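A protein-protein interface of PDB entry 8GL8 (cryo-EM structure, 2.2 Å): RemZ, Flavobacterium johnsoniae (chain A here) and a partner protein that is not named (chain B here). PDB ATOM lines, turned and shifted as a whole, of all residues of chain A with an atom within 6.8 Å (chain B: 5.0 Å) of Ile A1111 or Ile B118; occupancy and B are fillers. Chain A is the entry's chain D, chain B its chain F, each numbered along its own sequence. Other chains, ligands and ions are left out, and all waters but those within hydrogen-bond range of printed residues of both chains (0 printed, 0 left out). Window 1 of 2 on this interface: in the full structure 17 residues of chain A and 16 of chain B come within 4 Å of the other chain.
The backbone carbonyl oxygen of Phe B115 lies within hydrogen-bond range of the side-chain amino group of Lys A1110.
Of the 16 printed residues of chain A, 4 touch a printed residue of chain B. Hydrophobic or aromatic side chains of chain A within 4 Å of the printed part of chain B: Val A1094 and Val A1112. Among the printed residues, 6 pairs touch across the chains.
The backbone NH of Ile B118 is in hydrogen-bond range of the backbone carbonyl oxygen of Val B133 (2.9 Å). O of Arg B131 is in hydrogen-bond range of N of Leu B120 (2.9 Å). The backbone carbonyl oxygen (O) of Ile A1111 is in hydrogen-bond range of the backbone NH (N) of Leu A1095 (2.9 Å).
Among the printed residues, merely in contact across the chains: Val A1094 with Ile B118 (3.9 Å), Lys A1110 with Ile B118 (3.3 Å), Ile A1111 with Ile B118 (3.9 Å), Val A1112 with Ile B118 (3.8 Å) and Val A1112 with Leu B120 (3.6 Å).
Ile A1111 touches just one residue of chain B: Ile B118 (3.9 Å). Ile B118 touches four residues of chain A. Of the printed residues of chain B, Lys A1110 touches Phe B115 and Ile B118. Printed residues of chain B within 4 Å of Val A1094: Ile B118 (3.9 Å). Ile A1096 touches none of the printed residues of chain B.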
ATOM      1  N   VAL A1043      -7.940   1.631   6.705  1.00  0.00           N
ATOM      2  CA  VAL A1043      -7.468   0.388   6.107  1.00  0.00           C
ATOM      3  C   VAL A1043      -7.495   0.565   4.598  1.00  0.00           C
ATOM      4  O   VAL A1043      -8.530   0.934   4.031  1.00  0.00           O
ATOM      5  CB  VAL A1043      -8.321  -0.820   6.534  1.00  0.00           C
ATOM      6  CG1 VAL A1043      -7.666  -2.112   6.078  1.00  0.00           C
ATOM      7  CG2 VAL A1043      -8.524  -0.828   8.039  1.00  0.00           C
ATOM      8  N   SER A1044      -6.364   0.307   3.949  1.00  0.00           N
ATOM      9  CA  SER A1044      -6.231   0.507   2.514  1.00  0.00           C
ATOM     10  C   SER A1044      -5.771  -0.778   1.841  1.00  0.00           C
ATOM     11  O   SER A1044      -4.937  -1.510   2.379  1.00  0.00           O
ATOM     12  CB  SER A1044      -5.254   1.645   2.203  1.00  0.00           C
ATOM     13  OG  SER A1044      -4.033   1.484   2.903  1.00  0.00           O
ATOM     14  N   VAL A1045      -6.330  -1.055   0.666  1.00  0.00           N
ATOM     15  CA  VAL A1045      -5.947  -2.207  -0.142  1.00  0.00           C
ATOM     16  C   VAL A1045      -5.592  -1.698  -1.530  1.00  0.00           C
ATOM     17  O   VAL A1045      -6.449  -1.142  -2.228  1.00  0.00           O
ATOM     18  CB  VAL A1045      -7.068  -3.258  -0.223  1.00  0.00           C
ATOM     19  CG1 VAL A1045      -6.532  -4.567  -0.779  1.00  0.00           C
ATOM     20  CG2 VAL A1045      -7.702  -3.476   1.142  1.00  0.00           C
ATOM     21  N   ILE A1050      -2.956  -5.438   2.474  1.00  0.00           N
ATOM     22  CA  ILE A1050      -3.735  -4.672   3.440  1.00  0.00           C
ATOM     23  C   ILE A1050      -2.788  -3.781   4.229  1.00  0.00           C
ATOM     24  O   ILE A1050      -1.727  -4.229   4.674  1.00  0.00           O
ATOM     25  CB  ILE A1050      -4.538  -5.600   4.367  1.00  0.00           C
ATOM     26  CG1 ILE A1050      -5.575  -6.378   3.556  1.00  0.00           C
ATOM     27  CG2 ILE A1050      -5.213  -4.806   5.471  1.00  0.00           C
ATOM     28  CD1 ILE A1050      -6.102  -7.605   4.251  1.00  0.00           C
ATOM     29  N   ILE A1064      -8.237 -10.895  10.471  1.00  0.00           N
ATOM     30  CA  ILE A1064      -8.984 -10.707   9.235  1.00  0.00           C
ATOM     31  C   ILE A1064      -9.880 -11.920   9.046  1.00  0.00           C
ATOM     32  O   ILE A1064      -9.390 -13.057   8.991  1.00  0.00           O
ATOM     33  CB  ILE A1064      -8.058 -10.504   8.026  1.00  0.00           C
ATOM     34  CG1 ILE A1064      -7.321  -9.170   8.148  1.00  0.00           C
ATOM     35  CG2 ILE A1064      -8.856 -10.540   6.735  1.00  0.00           C
ATOM     36  CD1 ILE A1064      -5.878  -9.228   7.726  1.00  0.00           C
ATOM     37  N   ILE A1067     -16.581 -13.163   5.138  1.00  0.00           N
ATOM     38  CA  ILE A1067     -18.010 -12.959   5.355  1.00  0.00           C
ATOM     39  C   ILE A1067     -18.639 -14.202   5.970  1.00  0.00           C
ATOM     40  O   ILE A1067     -19.600 -14.108   6.741  1.00  0.00           O
ATOM     41  CB  ILE A1067     -18.686 -12.549   4.031  1.00  0.00           C
ATOM     42  CG1 ILE A1067     -18.439 -11.065   3.756  1.00  0.00           C
ATOM     43  CG2 ILE A1067     -20.180 -12.836   4.051  1.00  0.00           C
ATOM     44  CD1 ILE A1067     -18.710 -10.177   4.953  1.00  0.00           C
ATOM     45  N   GLN A1093     -14.576 -11.143  -1.838  1.00  0.00           N
ATOM     46  CA  GLN A1093     -13.969  -9.819  -1.881  1.00  0.00           C
ATOM     47  C   GLN A1093     -14.081  -9.074  -0.563  1.00  0.00           C
ATOM     48  O   GLN A1093     -13.126  -8.416  -0.146  1.00  0.00           O
ATOM     49  CB  GLN A1093     -14.616  -8.978  -2.991  1.00  0.00           C
ATOM     50  CG  GLN A1093     -14.639  -9.643  -4.355  1.00  0.00           C
ATOM     51  CD  GLN A1093     -15.457  -8.863  -5.368  1.00  0.00           C
ATOM     52  OE1 GLN A1093     -16.681  -8.975  -5.412  1.00  0.00           O
ATOM     53  NE2 GLN A1093     -14.782  -8.065  -6.185  1.00  0.00           N
ATOM     54  N   VAL A1094     -15.225  -9.163   0.100  1.00  0.00           N
ATOM     55  CA  VAL A1094     -15.465  -8.463   1.360  1.00  0.00           C
ATOM     56  C   VAL A1094     -14.762  -9.182   2.504  1.00  0.00           C
ATOM     57  O   VAL A1094     -14.906 -10.398   2.678  1.00  0.00           O
ATOM     58  CB  VAL A1094     -16.971  -8.329   1.630  1.00  0.00           C
ATOM     59  CG1 VAL A1094     -17.210  -7.553   2.914  1.00  0.00           C
ATOM     60  CG2 VAL A1094     -17.658  -7.648   0.460  1.00  0.00           C
ATOM     61  N   LEU A1095     -14.006  -8.422   3.293  1.00  0.00           N
ATOM     62  CA  LEU A1095     -13.293  -8.917   4.460  1.00  0.00           C
ATOM     63  C   LEU A1095     -13.568  -8.003   5.646  1.00  0.00           C
ATOM     64  O   LEU A1095     -13.901  -6.826   5.487  1.00  0.00           O
ATOM     65  CB  LEU A1095     -11.783  -8.989   4.211  1.00  0.00           C
ATOM     66  CG  LEU A1095     -11.318  -9.919   3.096  1.00  0.00           C
ATOM     67  CD1 LEU A1095      -9.815  -9.830   2.934  1.00  0.00           C
ATOM     68  CD2 LEU A1095     -11.745 -11.336   3.401  1.00  0.00           C
ATOM     69  N   ILE A1096     -13.414  -8.558   6.847  1.00  0.00           N
ATOM     70  CA  ILE A1096     -13.601  -7.816   8.088  1.00  0.00           C
ATOM     71  C   ILE A1096     -12.277  -7.792   8.838  1.00  0.00           C
ATOM     72  O   ILE A1096     -11.695  -8.847   9.111  1.00  0.00           O
ATOM     73  CB  ILE A1096     -14.714  -8.432   8.956  1.00  0.00           C
ATOM     74  CG1 ILE A1096     -16.059  -8.348   8.233  1.00  0.00           C
ATOM     75  CG2 ILE A1096     -14.792  -7.731  10.300  1.00  0.00           C
ATOM     76  CD1 ILE A1096     -17.035  -9.431   8.627  1.00  0.00           C
ATOM     77  N   VAL A1097     -11.806  -6.595   9.171  1.00  0.00           N
ATOM     78  CA  VAL A1097     -10.551  -6.398   9.883  1.00  0.00           C
ATOM     79  C   VAL A1097     -10.882  -5.924  11.291  1.00  0.00           C
ATOM     80  O   VAL A1097     -11.529  -4.884  11.470  1.00  0.00           O
ATOM     81  CB  VAL A1097      -9.641  -5.390   9.162  1.00  0.00           C
ATOM     82  CG1 VAL A1097      -8.285  -5.314   9.845  1.00  0.00           C
ATOM     83  CG2 VAL A1097      -9.487  -5.766   7.697  1.00  0.00           C
ATOM     84  N   LYS A1109     -13.351  -2.728  10.699  1.00  0.00           N
ATOM     85  CA  LYS A1109     -13.407  -2.125   9.375  1.00  0.00           C
ATOM     86  C   LYS A1109     -13.768  -3.177   8.339  1.00  0.00           C
ATOM     87  O   LYS A1109     -13.157  -4.245   8.295  1.00  0.00           O
ATOM     88  CB  LYS A1109     -12.072  -1.466   9.011  1.00  0.00           C
ATOM     89  CG  LYS A1109     -12.199  -0.329   8.011  1.00  0.00           C
ATOM     90  CD  LYS A1109     -12.800   0.916   8.649  1.00  0.00           C
ATOM     91  CE  LYS A1109     -12.153   1.230   9.987  1.00  0.00           C
ATOM     92  NZ  LYS A1109     -12.384   2.644  10.394  1.00  0.00           N
ATOM     93  N   LYS A1110     -14.750  -2.870   7.501  1.00  0.00           N
ATOM     94  CA  LYS A1110     -15.091  -3.714   6.367  1.00  0.00           C
ATOM     95  C   LYS A1110     -14.350  -3.205   5.139  1.00  0.00           C
ATOM     96  O   LYS A1110     -14.423  -2.016   4.814  1.00  0.00           O
ATOM     97  CB  LYS A1110     -16.599  -3.723   6.119  1.00  0.00           C
ATOM     98  CG  LYS A1110     -17.312  -4.914   6.730  1.00  0.00           C
ATOM     99  CD  LYS A1110     -18.819  -4.787   6.600  1.00  0.00           C
ATOM    100  CE  LYS A1110     -19.346  -3.610   7.401  1.00  0.00           C
ATOM    101  NZ  LYS A1110     -20.728  -3.855   7.895  1.00  0.00           N
ATOM    102  N   ILE A1111     -13.623  -4.100   4.470  1.00  0.00           N
ATOM    103  CA  ILE A1111     -12.830  -3.742   3.303  1.00  0.00           C
ATOM    104  C   ILE A1111     -13.193  -4.671   2.154  1.00  0.00           C
ATOM    105  O   ILE A1111     -13.811  -5.719   2.341  1.00  0.00           O
ATOM    106  CB  ILE A1111     -11.310  -3.802   3.576  1.00  0.00           C
ATOM    107  CG1 ILE A1111     -10.829  -5.254   3.607  1.00  0.00           C
ATOM    108  CG2 ILE A1111     -10.966  -3.088   4.873  1.00  0.00           C
ATOM    109  CD1 ILE A1111      -9.363  -5.406   3.931  1.00  0.00           C
ATOM    110  N   VAL A1112     -12.805  -4.264   0.951  1.00  0.00           N
ATOM    111  CA  VAL A1112     -12.954  -5.080  -0.247  1.00  0.00           C
ATOM    112  C   VAL A1112     -11.561  -5.487  -0.701  1.00  0.00           C
ATOM    113  O   VAL A1112     -10.712  -4.630  -0.972  1.00  0.00           O
ATOM    114  CB  VAL A1112     -13.711  -4.334  -1.356  1.00  0.00           C
ATOM    115  CG1 VAL A1112     -13.545  -5.051  -2.683  1.00  0.00           C
ATOM    116  CG2 VAL A1112     -15.182  -4.213  -0.999  1.00  0.00           C
ATOM    117  N   PHE A1113     -11.324  -6.793  -0.777  1.00  0.00           N
ATOM    118  CA  PHE A1113     -10.008  -7.323  -1.121  1.00  0.00           C
ATOM    119  C   PHE A1113      -9.811  -7.230  -2.628  1.00  0.00           C
ATOM    120  O   PHE A1113     -10.415  -7.990  -3.390  1.00  0.00           O
ATOM    121  CB  PHE A1113      -9.875  -8.762  -0.635  1.00  0.00           C
ATOM    122  CG  PHE A1113      -8.458  -9.192  -0.396  1.00  0.00           C
ATOM    123  CD1 PHE A1113      -7.536  -8.315   0.145  1.00  0.00           C
ATOM    124  CD2 PHE A1113      -8.050 -10.478  -0.708  1.00  0.00           C
ATOM    125  CE1 PHE A1113      -6.231  -8.709   0.367  1.00  0.00           C
ATOM    126  CE2 PHE A1113      -6.748 -10.879  -0.486  1.00  0.00           C
ATOM    127  CZ  PHE A1113      -5.837  -9.993   0.051  1.00  0.00           C
ATOM    128  N   PHE B 115     -24.442  -5.729   3.433  1.00  0.00           N
ATOM    129  CA  PHE B 115     -23.241  -5.635   4.248  1.00  0.00           C
ATOM    130  C   PHE B 115     -23.002  -4.228   4.773  1.00  0.00           C
ATOM    131  O   PHE B 115     -22.023  -4.008   5.492  1.00  0.00           O
ATOM    132  CB  PHE B 115     -22.017  -6.087   3.447  1.00  0.00           C
ATOM    133  CG  PHE B 115     -22.143  -7.464   2.866  1.00  0.00           C
ATOM    134  CD1 PHE B 115     -22.599  -8.517   3.637  1.00  0.00           C
ATOM    135  CD2 PHE B 115     -21.798  -7.706   1.549  1.00  0.00           C
ATOM    136  CE1 PHE B 115     -22.712  -9.785   3.102  1.00  0.00           C
ATOM    137  CE2 PHE B 115     -21.909  -8.970   1.010  1.00  0.00           C
ATOM    138  CZ  PHE B 115     -22.366 -10.012   1.788  1.00  0.00           C
ATOM    139  N   GLY B 116     -23.865  -3.275   4.435  1.00  0.00           N
ATOM    140  CA  GLY B 116     -23.631  -1.889   4.772  1.00  0.00           C
ATOM    141  C   GLY B 116     -22.647  -1.241   3.818  1.00  0.00           C
ATOM    142  O   GLY B 116     -22.140  -1.848   2.874  1.00  0.00           O
ATOM    143  N   GLY B 117     -22.378   0.035   4.077  1.00  0.00           N
ATOM    144  CA  GLY B 117     -21.424   0.760   3.258  1.00  0.00           C
ATOM    145  C   GLY B 117     -20.002   0.294   3.517  1.00  0.00           C
ATOM    146  O   GLY B 117     -19.578   0.122   4.661  1.00  0.00           O
ATOM    147  N   ILE B 118     -19.262   0.080   2.434  1.00  0.00           N
ATOM    148  CA  ILE B 118     -17.855  -0.294   2.493  1.00  0.00           C
ATOM    149  C   ILE B 118     -17.073   0.717   1.669  1.00  0.00           C
ATOM    150  O   ILE B 118     -17.371   0.925   0.487  1.00  0.00           O
ATOM    151  CB  ILE B 118     -17.615  -1.723   1.980  1.00  0.00           C
ATOM    152  CG1 ILE B 118     -18.413  -2.732   2.807  1.00  0.00           C
ATOM    153  CG2 ILE B 118     -16.133  -2.058   2.016  1.00  0.00           C
ATOM    154  CD1 ILE B 118     -18.636  -4.053   2.109  1.00  0.00           C
ATOM    155  N   GLU B 119     -16.078   1.342   2.290  1.00  0.00           N
ATOM    156  CA  GLU B 119     -15.259   2.343   1.623  1.00  0.00           C
ATOM    157  C   GLU B 119     -14.080   1.668   0.935  1.00  0.00           C
ATOM    158  O   GLU B 119     -13.381   0.855   1.545  1.00  0.00           O
ATOM    159  CB  GLU B 119     -14.762   3.382   2.629  1.00  0.00           C
ATOM    160  CG  GLU B 119     -14.579   4.772   2.052  1.00  0.00           C
ATOM    161  CD  GLU B 119     -15.898   5.476   1.796  1.00  0.00           C
ATOM    162  OE1 GLU B 119     -16.905   5.102   2.434  1.00  0.00           O
ATOM    163  OE2 GLU B 119     -15.930   6.402   0.959  1.00  0.00           O
ATOM    164  N   LEU B 120     -13.866   2.002  -0.336  1.00  0.00           N
ATOM    165  CA  LEU B 120     -12.732   1.496  -1.099  1.00  0.00           C
ATOM    166  C   LEU B 120     -11.616   2.526  -1.001  1.00  0.00           C
ATOM    167  O   LEU B 120     -11.741   3.639  -1.519  1.00  0.00           O
ATOM    168  CB  LEU B 120     -13.121   1.242  -2.553  1.00  0.00           C
ATOM    169  CG  LEU B 120     -14.324   0.334  -2.821  1.00  0.00           C
ATOM    170  CD1 LEU B 120     -14.263  -0.222  -4.230  1.00  0.00           C
ATOM    171  CD2 LEU B 120     -14.388  -0.793  -1.811  1.00  0.00           C
ATOM    172  N   ARG B 131     -14.668   5.933  -2.866  1.00  0.00           N
ATOM    173  CA  ARG B 131     -15.884   5.347  -3.410  1.00  0.00           C
ATOM    174  C   ARG B 131     -16.480   4.377  -2.399  1.00  0.00           C
ATOM    175  O   ARG B 131     -15.780   3.500  -1.883  1.00  0.00           O
ATOM    176  CB  ARG B 131     -15.590   4.631  -4.730  1.00  0.00           C
ATOM    177  CG  ARG B 131     -16.792   3.963  -5.367  1.00  0.00           C
ATOM    178  CD  ARG B 131     -16.409   3.286  -6.672  1.00  0.00           C
ATOM    179  NE  ARG B 131     -14.994   2.931  -6.705  1.00  0.00           N
ATOM    180  CZ  ARG B 131     -14.527   1.747  -7.077  1.00  0.00           C
ATOM    181  NH1 ARG B 131     -15.337   0.773  -7.458  1.00  0.00           N
ATOM    182  NH2 ARG B 131     -13.214   1.535  -7.064  1.00  0.00           N
ATOM    183  N   GLU B 132     -17.771   4.523  -2.127  1.00  0.00           N
ATOM    184  CA  GLU B 132     -18.473   3.638  -1.210  1.00  0.00           C
ATOM    185  C   GLU B 132     -19.339   2.669  -2.004  1.00  0.00           C
ATOM    186  O   GLU B 132     -20.119   3.087  -2.866  1.00  0.00           O
ATOM    187  CB  GLU B 132     -19.329   4.433  -0.224  1.00  0.00           C
ATOM    188  CG  GLU B 132     -20.281   3.578   0.596  1.00  0.00           C
ATOM    189  CD  GLU B 132     -20.277   3.944   2.066  1.00  0.00           C
ATOM    190  OE1 GLU B 132     -19.306   3.590   2.766  1.00  0.00           O
ATOM    191  OE2 GLU B 132     -21.247   4.585   2.522  1.00  0.00           O
ATOM    192  N   VAL B 133     -19.194   1.380  -1.715  1.00  0.00           N
ATOM    193  CA  VAL B 133     -19.981   0.337  -2.357  1.00  0.00           C
ATOM    194  C   VAL B 133     -20.867  -0.316  -1.307  1.00  0.00           C
ATOM    195  O   VAL B 133     -20.503  -0.421  -0.131  1.00  0.00           O
ATOM    196  CB  VAL B 133     -19.094  -0.714  -3.059  1.00  0.00           C
ATOM    197  CG1 VAL B 133     -18.285  -0.067  -4.168  1.00  0.00           C
ATOM    198  CG2 VAL B 133     -18.179  -1.401  -2.056  1.00  0.00           C
ATOM    199  N   PRO B 135     -22.697  -3.777  -1.517  1.00  0.00           N
ATOM    200  CA  PRO B 135     -23.150  -5.052  -2.091  1.00  0.00           C
ATOM    201  C   PRO B 135     -24.391  -5.542  -1.363  1.00  0.00           C
ATOM    202  O   PRO B 135     -24.420  -5.613  -0.133  1.00  0.00           O
ATOM    203  CB  PRO B 135     -21.957  -5.990  -1.874  1.00  0.00           C
ATOM    204  CG  PRO B 135     -20.824  -5.129  -1.416  1.00  0.00           C
ATOM    205  CD  PRO B 135     -21.408  -3.902  -0.820  1.00  0.00           C
